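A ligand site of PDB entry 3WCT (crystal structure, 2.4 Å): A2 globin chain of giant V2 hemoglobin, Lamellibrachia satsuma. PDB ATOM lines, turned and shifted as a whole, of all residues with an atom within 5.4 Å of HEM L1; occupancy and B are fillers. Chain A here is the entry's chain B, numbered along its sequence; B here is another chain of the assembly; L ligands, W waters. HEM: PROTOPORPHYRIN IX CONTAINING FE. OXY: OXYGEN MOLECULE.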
ATOM      1  N   TRP A  33     -35.955 -30.134  24.602  1.00  0.00           N
ATOM      2  CA  TRP A  33     -35.660 -29.205  23.519  1.00  0.00           C
ATOM      3  C   TRP A  33     -36.344 -29.509  22.199  1.00  0.00           C
ATOM      4  O   TRP A  33     -36.477 -28.614  21.356  1.00  0.00           O
ATOM      5  CB  TRP A  33     -34.154 -29.055  23.346  1.00  0.00           C
ATOM      6  CG  TRP A  33     -33.584 -28.216  24.438  1.00  0.00           C
ATOM      7  CD1 TRP A  33     -33.096 -28.650  25.651  1.00  0.00           C
ATOM      8  CD2 TRP A  33     -33.568 -26.784  24.491  1.00  0.00           C
ATOM      9  NE1 TRP A  33     -32.790 -27.570  26.450  1.00  0.00           N
ATOM     10  CE2 TRP A  33     -33.068 -26.414  25.760  1.00  0.00           C
ATOM     11  CE3 TRP A  33     -33.931 -25.774  23.587  1.00  0.00           C
ATOM     12  CZ2 TRP A  33     -32.923 -25.086  26.155  1.00  0.00           C
ATOM     13  CZ3 TRP A  33     -33.792 -24.450  23.975  1.00  0.00           C
ATOM     14  CH2 TRP A  33     -33.290 -24.111  25.250  1.00  0.00           C
ATOM     15  N   ALA A  43     -37.325 -19.416  17.913  1.00  0.00           N
ATOM     16  CA  ALA A  43     -36.279 -19.306  18.914  1.00  0.00           C
ATOM     17  C   ALA A  43     -34.931 -19.967  18.622  1.00  0.00           C
ATOM     18  O   ALA A  43     -33.921 -19.537  19.161  1.00  0.00           O
ATOM     19  CB  ALA A  43     -36.803 -19.813  20.243  1.00  0.00           C
ATOM     20  N   MET A  46     -31.499 -18.126  18.148  1.00  0.00           N
ATOM     21  CA  MET A  46     -30.649 -17.643  19.235  1.00  0.00           C
ATOM     22  C   MET A  46     -29.549 -18.647  19.614  1.00  0.00           C
ATOM     23  O   MET A  46     -28.613 -18.310  20.333  1.00  0.00           O
ATOM     24  CB  MET A  46     -31.495 -17.369  20.478  1.00  0.00           C
ATOM     25  CG  MET A  46     -32.413 -16.170  20.329  1.00  0.00           C
ATOM     26  SD  MET A  46     -33.469 -15.982  21.762  1.00  0.00           S
ATOM     27  CE  MET A  46     -32.232 -15.960  23.070  1.00  0.00           C
ATOM     28  N   PHE A  47     -29.661 -19.870  19.097  1.00  0.00           N
ATOM     29  CA  PHE A  47     -28.709 -20.922  19.398  1.00  0.00           C
ATOM     30  C   PHE A  47     -27.739 -21.237  18.257  1.00  0.00           C
ATOM     31  O   PHE A  47     -27.266 -22.366  18.142  1.00  0.00           O
ATOM     32  CB  PHE A  47     -29.460 -22.179  19.814  1.00  0.00           C
ATOM     33  CG  PHE A  47     -30.303 -22.004  21.036  1.00  0.00           C
ATOM     34  CD1 PHE A  47     -29.750 -22.119  22.306  1.00  0.00           C
ATOM     35  CD2 PHE A  47     -31.638 -21.652  20.931  1.00  0.00           C
ATOM     36  CE1 PHE A  47     -30.504 -21.895  23.443  1.00  0.00           C
ATOM     37  CE2 PHE A  47     -32.408 -21.424  22.064  1.00  0.00           C
ATOM     38  CZ  PHE A  47     -31.839 -21.539  23.321  1.00  0.00           C
ATOM     39  N   ARG A  49     -24.622 -20.596  17.829  1.00  0.00           N
ATOM     40  CA  ARG A  49     -23.324 -21.091  18.284  1.00  0.00           C
ATOM     41  C   ARG A  49     -23.316 -22.533  18.783  1.00  0.00           C
ATOM     42  O   ARG A  49     -22.254 -23.165  18.817  1.00  0.00           O
ATOM     43  CB  ARG A  49     -22.758 -20.171  19.381  1.00  0.00           C
ATOM     44  CG  ARG A  49     -21.256 -20.329  19.623  1.00  0.00           C
ATOM     45  CD  ARG A  49     -20.813 -19.537  20.831  1.00  0.00           C
ATOM     46  NE  ARG A  49     -21.381 -20.088  22.064  1.00  0.00           N
ATOM     47  CZ  ARG A  49     -20.944 -21.206  22.645  1.00  0.00           C
ATOM     48  NH1 ARG A  49     -19.931 -21.887  22.116  1.00  0.00           N
ATOM     49  NH2 ARG A  49     -21.544 -21.658  23.742  1.00  0.00           N
ATOM     50  N   VAL A  50     -24.473 -23.049  19.187  1.00  0.00           N
ATOM     51  CA  VAL A  50     -24.526 -24.419  19.688  1.00  0.00           C
ATOM     52  C   VAL A  50     -25.342 -25.348  18.806  1.00  0.00           C
ATOM     53  O   VAL A  50     -25.942 -26.318  19.273  1.00  0.00           O
ATOM     54  CB  VAL A  50     -25.041 -24.453  21.151  1.00  0.00           C
ATOM     55  CG1 VAL A  50     -24.207 -23.507  22.006  1.00  0.00           C
ATOM     56  CG2 VAL A  50     -26.500 -24.085  21.224  1.00  0.00           C
ATOM     57  N   HIS A  63     -24.963 -28.247  25.206  1.00  0.00           N
ATOM     58  CA  HIS A  63     -25.728 -27.092  25.671  1.00  0.00           C
ATOM     59  C   HIS A  63     -26.924 -27.584  26.520  1.00  0.00           C
ATOM     60  O   HIS A  63     -27.141 -27.092  27.637  1.00  0.00           O
ATOM     61  CB  HIS A  63     -26.242 -26.257  24.479  1.00  0.00           C
ATOM     62  CG  HIS A  63     -27.313 -25.281  24.844  1.00  0.00           C
ATOM     63  ND1 HIS A  63     -27.044 -24.108  25.517  1.00  0.00           N
ATOM     64  CD2 HIS A  63     -28.662 -25.341  24.718  1.00  0.00           C
ATOM     65  CE1 HIS A  63     -28.184 -23.490  25.793  1.00  0.00           C
ATOM     66  NE2 HIS A  63     -29.186 -24.221  25.314  1.00  0.00           N
ATOM     67  N   ARG A  66     -25.780 -28.415  29.758  1.00  0.00           N
ATOM     68  CA  ARG A  66     -25.571 -27.242  30.607  1.00  0.00           C
ATOM     69  C   ARG A  66     -26.867 -26.697  31.168  1.00  0.00           C
ATOM     70  O   ARG A  66     -26.960 -26.425  32.366  1.00  0.00           O
ATOM     71  CB  ARG A  66     -24.844 -26.133  29.848  1.00  0.00           C
ATOM     72  CG  ARG A  66     -23.396 -26.464  29.530  1.00  0.00           C
ATOM     73  CD  ARG A  66     -22.615 -25.229  29.042  1.00  0.00           C
ATOM     74  NE  ARG A  66     -23.040 -24.778  27.716  1.00  0.00           N
ATOM     75  CZ  ARG A  66     -22.675 -25.335  26.576  1.00  0.00           C
ATOM     76  NH1 ARG A  66     -23.123 -24.839  25.421  1.00  0.00           N
ATOM     77  NH2 ARG A  66     -21.857 -26.381  26.550  1.00  0.00           N
ATOM     78  N   VAL A  67     -27.874 -26.539  30.303  1.00  0.00           N
ATOM     79  CA  VAL A  67     -29.181 -26.007  30.713  1.00  0.00           C
ATOM     80  C   VAL A  67     -29.806 -26.814  31.849  1.00  0.00           C
ATOM     81  O   VAL A  67     -30.233 -26.246  32.854  1.00  0.00           O
ATOM     82  CB  VAL A  67     -30.187 -26.010  29.537  1.00  0.00           C
ATOM     83  CG1 VAL A  67     -31.576 -25.588  30.041  1.00  0.00           C
ATOM     84  CG2 VAL A  67     -29.709 -25.091  28.452  1.00  0.00           C
ATOM     85  N   GLY A  70     -28.343 -26.340  34.916  1.00  0.00           N
ATOM     86  CA  GLY A  70     -28.746 -25.069  35.507  1.00  0.00           C
ATOM     87  C   GLY A  70     -30.046 -25.242  36.276  1.00  0.00           C
ATOM     88  O   GLY A  70     -30.198 -24.742  37.391  1.00  0.00           O
ATOM     89  N   LEU A  71     -30.978 -25.958  35.677  1.00  0.00           N
ATOM     90  CA  LEU A  71     -32.255 -26.223  36.325  1.00  0.00           C
ATOM     91  C   LEU A  71     -32.027 -27.025  37.596  1.00  0.00           C
ATOM     92  O   LEU A  71     -32.713 -26.805  38.598  1.00  0.00           O
ATOM     93  CB  LEU A  71     -33.156 -27.029  35.398  1.00  0.00           C
ATOM     94  CG  LEU A  71     -34.161 -26.266  34.561  1.00  0.00           C
ATOM     95  CD1 LEU A  71     -34.844 -27.214  33.589  1.00  0.00           C
ATOM     96  CD2 LEU A  71     -35.166 -25.613  35.485  1.00  0.00           C
ATOM     97  N   CYS A  74     -30.901 -24.880  40.535  1.00  0.00           N
ATOM     98  CA  CYS A  74     -32.018 -24.132  41.062  1.00  0.00           C
ATOM     99  C   CYS A  74     -32.972 -25.022  41.864  1.00  0.00           C
ATOM    100  O   CYS A  74     -33.432 -24.630  42.935  1.00  0.00           O
ATOM    101  CB  CYS A  74     -32.778 -23.431  39.929  1.00  0.00           C
ATOM    102  SG  CYS A  74     -31.748 -22.314  38.939  1.00  0.00           S
ATOM    103  N   LEU A  91     -27.436 -16.880  36.529  1.00  0.00           N
ATOM    104  CA  LEU A  91     -28.108 -17.270  35.290  1.00  0.00           C
ATOM    105  C   LEU A  91     -28.616 -16.025  34.557  1.00  0.00           C
ATOM    106  O   LEU A  91     -28.601 -15.966  33.339  1.00  0.00           O
ATOM    107  CB  LEU A  91     -29.286 -18.199  35.602  1.00  0.00           C
ATOM    108  CG  LEU A  91     -28.965 -19.663  35.899  1.00  0.00           C
ATOM    109  CD1 LEU A  91     -30.189 -20.339  36.481  1.00  0.00           C
ATOM    110  CD2 LEU A  91     -28.525 -20.357  34.624  1.00  0.00           C
ATOM    111  N   GLN A  94     -25.978 -14.581  32.532  1.00  0.00           N
ATOM    112  CA  GLN A  94     -25.593 -15.450  31.418  1.00  0.00           C
ATOM    113  C   GLN A  94     -26.571 -15.314  30.252  1.00  0.00           C
ATOM    114  O   GLN A  94     -26.283 -15.748  29.136  1.00  0.00           O
ATOM    115  CB  GLN A  94     -25.504 -16.914  31.861  1.00  0.00           C
ATOM    116  CG  GLN A  94     -24.371 -17.204  32.849  1.00  0.00           C
ATOM    117  CD  GLN A  94     -24.340 -18.648  33.299  1.00  0.00           C
ATOM    118  OE1 GLN A  94     -25.344 -19.179  33.790  1.00  0.00           O
ATOM    119  NE2 GLN A  94     -23.189 -19.301  33.145  1.00  0.00           N
ATOM    120  N   HIS A  95     -27.730 -14.705  30.521  1.00  0.00           N
ATOM    121  CA  HIS A  95     -28.773 -14.483  29.518  1.00  0.00           C
ATOM    122  C   HIS A  95     -29.057 -12.995  29.247  1.00  0.00           C
ATOM    123  O   HIS A  95     -29.873 -12.674  28.381  1.00  0.00           O
ATOM    124  CB  HIS A  95     -30.088 -15.132  29.946  1.00  0.00           C
ATOM    125  CG  HIS A  95     -30.060 -16.630  29.994  1.00  0.00           C
ATOM    126  ND1 HIS A  95     -29.350 -17.335  30.946  1.00  0.00           N
ATOM    127  CD2 HIS A  95     -30.656 -17.551  29.200  1.00  0.00           C
ATOM    128  CE1 HIS A  95     -29.516 -18.622  30.739  1.00  0.00           C
ATOM    129  NE2 HIS A  95     -30.307 -18.786  29.686  1.00  0.00           N
ATOM    130  N   ARG A  98     -28.788 -11.452  25.523  1.00  0.00           N
ATOM    131  CA  ARG A  98     -29.362 -12.328  24.507  1.00  0.00           C
ATOM    132  C   ARG A  98     -30.826 -12.054  24.163  1.00  0.00           C
ATOM    133  O   ARG A  98     -31.393 -12.698  23.278  1.00  0.00           O
ATOM    134  CB  ARG A  98     -29.178 -13.784  24.920  1.00  0.00           C
ATOM    135  CG  ARG A  98     -27.734 -14.110  25.290  1.00  0.00           C
ATOM    136  CD  ARG A  98     -27.586 -15.504  25.873  1.00  0.00           C
ATOM    137  NE  ARG A  98     -26.191 -15.794  26.229  1.00  0.00           N
ATOM    138  CZ  ARG A  98     -25.205 -15.956  25.344  1.00  0.00           C
ATOM    139  NH1 ARG A  98     -23.973 -16.224  25.769  1.00  0.00           N
ATOM    140  NH2 ARG A  98     -25.447 -15.882  24.039  1.00  0.00           N
ATOM    141  N   VAL A 100     -33.952 -12.591  25.762  1.00  0.00           N
ATOM    142  CA  VAL A 100     -34.928 -13.680  25.873  1.00  0.00           C
ATOM    143  C   VAL A 100     -36.231 -13.045  26.358  1.00  0.00           C
ATOM    144  O   VAL A 100     -36.228 -12.267  27.315  1.00  0.00           O
ATOM    145  CB  VAL A 100     -34.487 -14.769  26.904  1.00  0.00           C
ATOM    146  CG1 VAL A 100     -35.537 -15.883  26.962  1.00  0.00           C
ATOM    147  CG2 VAL A 100     -33.131 -15.341  26.523  1.00  0.00           C
ATOM    148  N   GLN A 104     -40.688 -16.769  25.751  1.00  0.00           N
ATOM    149  CA  GLN A 104     -39.811 -17.903  25.507  1.00  0.00           C
ATOM    150  C   GLN A 104     -39.494 -18.614  26.815  1.00  0.00           C
ATOM    151  O   GLN A 104     -39.286 -19.823  26.842  1.00  0.00           O
ATOM    152  CB  GLN A 104     -38.518 -17.434  24.818  1.00  0.00           C
ATOM    153  CG  GLN A 104     -38.764 -16.781  23.459  1.00  0.00           C
ATOM    154  CD  GLN A 104     -37.488 -16.284  22.794  1.00  0.00           C
ATOM    155  OE1 GLN A 104     -36.761 -15.465  23.363  1.00  0.00           O
ATOM    156  NE2 GLN A 104     -37.213 -16.772  21.591  1.00  0.00           N
ATOM    157  N   TYR A 105     -39.447 -17.860  27.917  1.00  0.00           N
ATOM    158  CA  TYR A 105     -39.165 -18.464  29.208  1.00  0.00           C
ATOM    159  C   TYR A 105     -40.310 -19.405  29.545  1.00  0.00           C
ATOM    160  O   TYR A 105     -40.080 -20.545  29.946  1.00  0.00           O
ATOM    161  CB  TYR A 105     -39.022 -17.390  30.294  1.00  0.00           C
ATOM    162  CG  TYR A 105     -37.611 -16.883  30.404  1.00  0.00           C
ATOM    163  CD1 TYR A 105     -36.582 -17.738  30.783  1.00  0.00           C
ATOM    164  CD2 TYR A 105     -37.287 -15.568  30.069  1.00  0.00           C
ATOM    165  CE1 TYR A 105     -35.261 -17.296  30.837  1.00  0.00           C
ATOM    166  CE2 TYR A 105     -35.962 -15.118  30.113  1.00  0.00           C
ATOM    167  CZ  TYR A 105     -34.957 -15.991  30.496  1.00  0.00           C
ATOM    168  OH  TYR A 105     -33.633 -15.579  30.509  1.00  0.00           O
ATOM    169  N   VAL A 108     -40.107 -22.760  27.511  1.00  0.00           N
ATOM    170  CA  VAL A 108     -39.186 -23.696  28.123  1.00  0.00           C
ATOM    171  C   VAL A 108     -39.777 -24.295  29.395  1.00  0.00           C
ATOM    172  O   VAL A 108     -39.530 -25.463  29.694  1.00  0.00           O
ATOM    173  CB  VAL A 108     -37.848 -22.991  28.397  1.00  0.00           C
ATOM    174  CG1 VAL A 108     -36.898 -23.906  29.165  1.00  0.00           C
ATOM    175  CG2 VAL A 108     -37.208 -22.589  27.057  1.00  0.00           C
ATOM    176  N   VAL A 112     -40.193 -28.128  29.931  1.00  0.00           N
ATOM    177  CA  VAL A 112     -39.635 -28.804  31.089  1.00  0.00           C
ATOM    178  C   VAL A 112     -40.672 -29.667  31.808  1.00  0.00           C
ATOM    179  O   VAL A 112     -40.389 -30.789  32.209  1.00  0.00           O
ATOM    180  CB  VAL A 112     -39.034 -27.808  32.099  1.00  0.00           C
ATOM    181  CG1 VAL A 112     -38.848 -28.484  33.452  1.00  0.00           C
ATOM    182  CG2 VAL A 112     -37.673 -27.299  31.580  1.00  0.00           C
ATOM    183  N   ILE A 137     -38.382 -19.589  39.373  1.00  0.00           N
ATOM    184  CA  ILE A 137     -37.062 -19.729  38.784  1.00  0.00           C
ATOM    185  C   ILE A 137     -36.785 -18.810  37.588  1.00  0.00           C
ATOM    186  O   ILE A 137     -35.782 -18.101  37.578  1.00  0.00           O
ATOM    187  CB  ILE A 137     -36.789 -21.197  38.409  1.00  0.00           C
ATOM    188  CG1 ILE A 137     -36.691 -22.038  39.686  1.00  0.00           C
ATOM    189  CG2 ILE A 137     -35.510 -21.301  37.571  1.00  0.00           C
ATOM    190  CD1 ILE A 137     -36.798 -23.553  39.485  1.00  0.00           C
ATOM    191  N   THR A 138     -37.653 -18.827  36.589  1.00  0.00           N
ATOM    192  CA  THR A 138     -37.465 -18.001  35.403  1.00  0.00           C
ATOM    193  C   THR A 138     -37.613 -16.525  35.754  1.00  0.00           C
ATOM    194  O   THR A 138     -36.859 -15.665  35.289  1.00  0.00           O
ATOM    195  CB  THR A 138     -38.482 -18.336  34.311  1.00  0.00           C
ATOM    196  OG1 THR A 138     -39.794 -18.084  34.810  1.00  0.00           O
ATOM    197  CG2 THR A 138     -38.369 -19.795  33.918  1.00  0.00           C
ATOM    198  N   ILE A 141     -34.494 -15.384  36.790  1.00  0.00           N
ATOM    199  CA  ILE A 141     -33.473 -15.354  35.749  1.00  0.00           C
ATOM    200  C   ILE A 141     -33.686 -14.124  34.869  1.00  0.00           C
ATOM    201  O   ILE A 141     -32.757 -13.679  34.187  1.00  0.00           O
ATOM    202  CB  ILE A 141     -33.514 -16.633  34.872  1.00  0.00           C
ATOM    203  CG1 ILE A 141     -33.241 -17.865  35.730  1.00  0.00           C
ATOM    204  CG2 ILE A 141     -32.478 -16.556  33.768  1.00  0.00           C
ATOM    205  CD1 ILE A 141     -33.317 -19.173  34.968  1.00  0.00           C
ATOM    206  N   HIS B  94     -16.069 -25.974  26.365  1.00  0.00           N
ATOM    207  CA  HIS B  94     -16.812 -24.864  26.920  1.00  0.00           C
ATOM    208  C   HIS B  94     -16.260 -24.497  28.297  1.00  0.00           C
ATOM    209  O   HIS B  94     -16.079 -23.325  28.621  1.00  0.00           O
ATOM    210  CB  HIS B  94     -18.284 -25.232  27.038  1.00  0.00           C
ATOM    211  CG  HIS B  94     -19.162 -24.097  27.465  1.00  0.00           C
ATOM    212  ND1 HIS B  94     -19.715 -23.215  26.564  1.00  0.00           N
ATOM    213  CD2 HIS B  94     -19.591 -23.710  28.680  1.00  0.00           C
ATOM    214  CE1 HIS B  94     -20.452 -22.332  27.218  1.00  0.00           C
ATOM    215  NE2 HIS B  94     -20.395 -22.613  28.503  1.00  0.00           N
ATOM    216  N   GLN B  98     -14.134 -21.163  29.761  1.00  0.00           N
ATOM    217  CA  GLN B  98     -14.597 -20.486  30.963  1.00  0.00           C
ATOM    218  C   GLN B  98     -13.478 -20.303  31.999  1.00  0.00           C
ATOM    219  O   GLN B  98     -13.644 -19.555  32.960  1.00  0.00           O
ATOM    220  CB  GLN B  98     -15.771 -21.250  31.594  1.00  0.00           C
ATOM    221  CG  GLN B  98     -17.060 -21.209  30.776  1.00  0.00           C
ATOM    222  CD  GLN B  98     -18.193 -21.962  31.454  1.00  0.00           C
ATOM    223  OE1 GLN B  98     -18.032 -23.120  31.837  1.00  0.00           O
ATOM    224  NE2 GLN B  98     -19.342 -21.315  31.594  1.00  0.00           N
HETATM  225  CHA HEM L   1     -27.335 -20.576  27.760  1.00  0.00           C
HETATM  226  CHB HEM L   1     -29.723 -22.214  31.537  1.00  0.00           C
HETATM  227  CHC HEM L   1     -33.885 -20.607  29.665  1.00  0.00           C
HETATM  228  CHD HEM L   1     -31.457 -19.114  25.789  1.00  0.00           C
HETATM  229  C1A HEM L   1     -27.611 -21.181  28.969  1.00  0.00           C
HETATM  230  C2A HEM L   1     -26.629 -21.761  29.799  1.00  0.00           C
HETATM  231  C3A HEM L   1     -27.309 -22.240  30.866  1.00  0.00           C
HETATM  232  C4A HEM L   1     -28.723 -21.939  30.702  1.00  0.00           C
HETATM  233  CMA HEM L   1     -26.733 -22.970  32.093  1.00  0.00           C
HETATM  234  CAA HEM L   1     -25.122 -21.838  29.549  1.00  0.00           C
HETATM  235  CBA HEM L   1     -24.431 -20.541  29.937  1.00  0.00           C
HETATM  236  CGA HEM L   1     -22.917 -20.483  29.703  1.00  0.00           C
HETATM  237  O1A HEM L   1     -22.160 -21.372  30.181  1.00  0.00           O
HETATM  238  O2A HEM L   1     -22.487 -19.559  29.054  1.00  0.00           O
HETATM  239  C1B HEM L   1     -31.093 -21.890  31.394  1.00  0.00           C
HETATM  240  C2B HEM L   1     -32.097 -22.196  32.394  1.00  0.00           C
HETATM  241  C3B HEM L   1     -33.327 -21.703  31.833  1.00  0.00           C
HETATM  242  C4B HEM L   1     -32.976 -21.170  30.563  1.00  0.00           C
HETATM  243  CMB HEM L   1     -31.877 -22.862  33.693  1.00  0.00           C
HETATM  244  CAB HEM L   1     -34.597 -21.787  32.525  1.00  0.00           C
HETATM  245  CBB HEM L   1     -35.622 -22.491  32.124  1.00  0.00           C
HETATM  246  C1C HEM L   1     -33.564 -20.095  28.421  1.00  0.00           C
HETATM  247  C2C HEM L   1     -34.587 -19.550  27.515  1.00  0.00           C
HETATM  248  C3C HEM L   1     -33.923 -19.157  26.343  1.00  0.00           C
HETATM  249  C4C HEM L   1     -32.461 -19.423  26.652  1.00  0.00           C
HETATM  250  CMC HEM L   1     -36.088 -19.466  27.802  1.00  0.00           C
HETATM  251  CAC HEM L   1     -34.474 -18.664  25.206  1.00  0.00           C
HETATM  252  CBC HEM L   1     -35.257 -19.077  24.253  1.00  0.00           C
HETATM  253  C1D HEM L   1     -30.101 -19.354  26.005  1.00  0.00           C
HETATM  254  C2D HEM L   1     -29.024 -18.971  25.022  1.00  0.00           C
HETATM  255  C3D HEM L   1     -27.860 -19.400  25.594  1.00  0.00           C
HETATM  256  C4D HEM L   1     -28.215 -20.013  26.896  1.00  0.00           C
HETATM  257  CMD HEM L   1     -29.281 -18.284  23.694  1.00  0.00           C
HETATM  258  CAD HEM L   1     -26.453 -19.261  25.029  1.00  0.00           C
HETATM  259  CBD HEM L   1     -25.996 -20.468  24.237  1.00  0.00           C
HETATM  260  CGD HEM L   1     -24.583 -20.348  23.803  1.00  0.00           C
HETATM  261  O1D HEM L   1     -23.663 -20.670  24.591  1.00  0.00           O
HETATM  262  O2D HEM L   1     -24.316 -19.947  22.658  1.00  0.00           O
HETATM  263  NA  HEM L   1     -28.904 -21.281  29.511  1.00  0.00           N
HETATM  264  NB  HEM L   1     -31.574 -21.269  30.314  1.00  0.00           N
HETATM  265  NC  HEM L   1     -32.299 -19.999  27.862  1.00  0.00           N
HETATM  266  ND  HEM L   1     -29.570 -19.943  27.093  1.00  0.00           N
HETATM  267 FE   HEM L   1     -30.591 -20.615  28.697  1.00  0.00          FE
HETATM  268  O1  OXY L   2     -30.811 -22.166  27.828  1.00  0.00           O
HETATM  269  O2  OXY L   2     -31.063 -22.566  26.696  1.00  0.00           O
HETATM  270  CHA HEM L   3     -15.374 -20.914  37.427  1.00  0.00           C
HETATM  271  CHB HEM L   3     -15.781 -25.632  37.167  1.00  0.00           C
HETATM  272  CHC HEM L   3     -11.218 -26.184  38.627  1.00  0.00           C
HETATM  273  CHD HEM L   3     -10.777 -21.383  38.690  1.00  0.00           C
HETATM  274  C1A HEM L   3     -15.895 -22.163  37.203  1.00  0.00           C
HETATM  275  C2A HEM L   3     -17.226 -22.386  36.800  1.00  0.00           C
HETATM  276  C3A HEM L   3     -17.338 -23.730  36.707  1.00  0.00           C
HETATM  277  C4A HEM L   3     -16.076 -24.340  37.081  1.00  0.00           C
HETATM  278  CMA HEM L   3     -18.591 -24.536  36.293  1.00  0.00           C
HETATM  279  CAA HEM L   3     -18.320 -21.358  36.550  1.00  0.00           C
HETATM  280  CBA HEM L   3     -18.412 -20.924  35.122  1.00  0.00           C
HETATM  281  CGA HEM L   3     -19.518 -19.901  34.842  1.00  0.00           C
HETATM  282  O1A HEM L   3     -20.713 -20.163  35.155  1.00  0.00           O
HETATM  283  O2A HEM L   3     -19.213 -18.870  34.319  1.00  0.00           O
HETATM  284  C1B HEM L   3     -14.571 -26.245  37.574  1.00  0.00           C
HETATM  285  C2B HEM L   3     -14.378 -27.679  37.673  1.00  0.00           C
HETATM  286  C3B HEM L   3     -13.016 -27.825  38.121  1.00  0.00           C
HETATM  287  C4B HEM L   3     -12.517 -26.506  38.236  1.00  0.00           C
HETATM  288  CMB HEM L   3     -15.379 -28.736  37.385  1.00  0.00           C
HETATM  289  CAB HEM L   3     -12.387 -29.114  38.381  1.00  0.00           C
HETATM  290  CBB HEM L   3     -11.744 -29.822  37.468  1.00  0.00           C
HETATM  291  C1C HEM L   3     -10.695 -24.892  38.742  1.00  0.00           C
HETATM  292  C2C HEM L   3      -9.298 -24.643  39.129  1.00  0.00           C
HETATM  293  C3C HEM L   3      -9.116 -23.242  39.147  1.00  0.00           C
HETATM  294  C4C HEM L   3     -10.500 -22.711  38.758  1.00  0.00           C
HETATM  295  CMC HEM L   3      -8.259 -25.708  39.440  1.00  0.00           C
HETATM  296  CAC HEM L   3      -7.974 -22.548  39.438  1.00  0.00           C
HETATM  297  CBC HEM L   3      -7.190 -22.321  40.434  1.00  0.00           C
HETATM  298  C1D HEM L   3     -12.006 -20.827  38.373  1.00  0.00           C
HETATM  299  C2D HEM L   3     -12.281 -19.346  38.390  1.00  0.00           C
HETATM  300  C3D HEM L   3     -13.608 -19.244  38.049  1.00  0.00           C
HETATM  301  C4D HEM L   3     -14.104 -20.615  37.815  1.00  0.00           C
HETATM  302  CMD HEM L   3     -11.251 -18.269  38.727  1.00  0.00           C
HETATM  303  CAD HEM L   3     -14.435 -17.985  37.943  1.00  0.00           C
HETATM  304  CBD HEM L   3     -15.207 -17.755  39.212  1.00  0.00           C
HETATM  305  CGD HEM L   3     -16.144 -16.638  39.125  1.00  0.00           C
HETATM  306  O1D HEM L   3     -15.772 -15.480  39.457  1.00  0.00           O
HETATM  307  O2D HEM L   3     -17.306 -16.857  38.735  1.00  0.00           O
HETATM  308  NA  HEM L   3     -15.173 -23.350  37.367  1.00  0.00           N
HETATM  309  NB  HEM L   3     -13.491 -25.523  37.898  1.00  0.00           N
HETATM  310  NC  HEM L   3     -11.374 -23.700  38.506  1.00  0.00           N
HETATM  311  ND  HEM L   3     -13.115 -21.527  38.043  1.00  0.00           N
HETATM  312 FE   HEM L   3     -13.267 -23.521  37.928  1.00  0.00          FE
HETATM  313  O   HOH W   1     -22.711 -23.192  32.222  1.00  0.00           O
HETATM  314  O   HOH W   2     -24.492 -22.933  26.196  1.00  0.00           O
HETATM  315  O   HOH W   3     -23.774 -16.574  29.011  1.00  0.00           O
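O1D of HEM L1 is in salt-bridge range of NH2 of Arg 49 (2.5 Å). An oxygen (O2) of OXY L2 lies within hydrogen-bond range of a ring nitrogen (NE2) of His 63 (2.9 Å). O1A of HEM L3 lies within hydrogen-bond range of NE2 of Gln 94 of chain A. A ring nitrogen (NE2) of His 95 is bound to an iron atom (FE) of HEM L1 (2.1 Å). The side-chain amide nitrogen of Gln 98 of chain B sits at hydrogen-bond distance from an oxygen (O1A) of HEM L1 (3.2 Å). A ring nitrogen (NE2) of His 94 of chain B lies within hydrogen-bond range of an oxygen (O1A) of HEM L1 (2.7 Å).
An iron atom (FE) of HEM L1 is bound by an oxygen (O1) of OXY L2, 1.8 Å away.
The backbone carbonyl oxygen of Leu 91 lies within hydrogen-bond range of a ring nitrogen (ND1) of His 95 (2.9 Å). The side-chain sulfur of Cys 74 is in hydrogen-bond range of the backbone carbonyl oxygen of Gly 70, 3.3 Å away. OE1 of Gln 104 sits close to SD of Met 46 (3.7 Å). NE of Arg 98 of chain A is in hydrogen-bond range of O of Gln 94 of chain A (2.9 Å).
Residues that only touch HEM L1: Met 46 (3.4 Å), Phe 47 (3.5 Å), Val 50 (3.6 Å), His 63 (3.6 Å), Arg 66 (3.5 Å), Val 67 (3.9 Å), Gly 70 (3.96 Å), Leu 71 (3.8 Å), Leu 91 (3.8 Å), Gln 94 of chain A (3.6 Å), Arg 98 of chain A (3.5 Å), Val 100 (3.5 Å), Gln 104 (3.4 Å), Tyr 105 (3.5 Å), Val 108 (3.4 Å) and Ile 141 (3.8 Å). Hydrophobic or aromatic side chains within 4 Å of HEM L1: Met 46, Phe 47, Val 50, His 63, Val 67, Leu 91, His 95, Val 100, Tyr 105, Val 108, Ile 141 and His 94 of chain B. Within 4 Å of HEM L1: Met 46, Phe 47, Arg 49, Val 50, His 63, Arg 66, Val 67, Gly 70, Leu 71, Leu 91, Gln 94 of chain A, His 95, Arg 98 of chain A, Val 100, Gln 104, Tyr 105, Val 108, Ile 141, His 94 of chain B and Gln 98 of chain B. Along chain A the residues within 4 Å of HEM L1 span positions 46 to 141. The nearest printed residue that does not touch HEM L1 is Thr 138 (4.2 Å).
Water W2 lies within hydrogen-bond range of NH1 of Arg 66 (2.5 Å), ND1 of His 63 (2.9 Å) and O1D of HEM L1 (2.9 Å). Water W3 lies within hydrogen-bond range of O of Gln 94 of chain A (2.6 Å), O2A of HEM L1 (3.3 Å) and NH1 of Arg 98 of chain A (3.3 Å).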
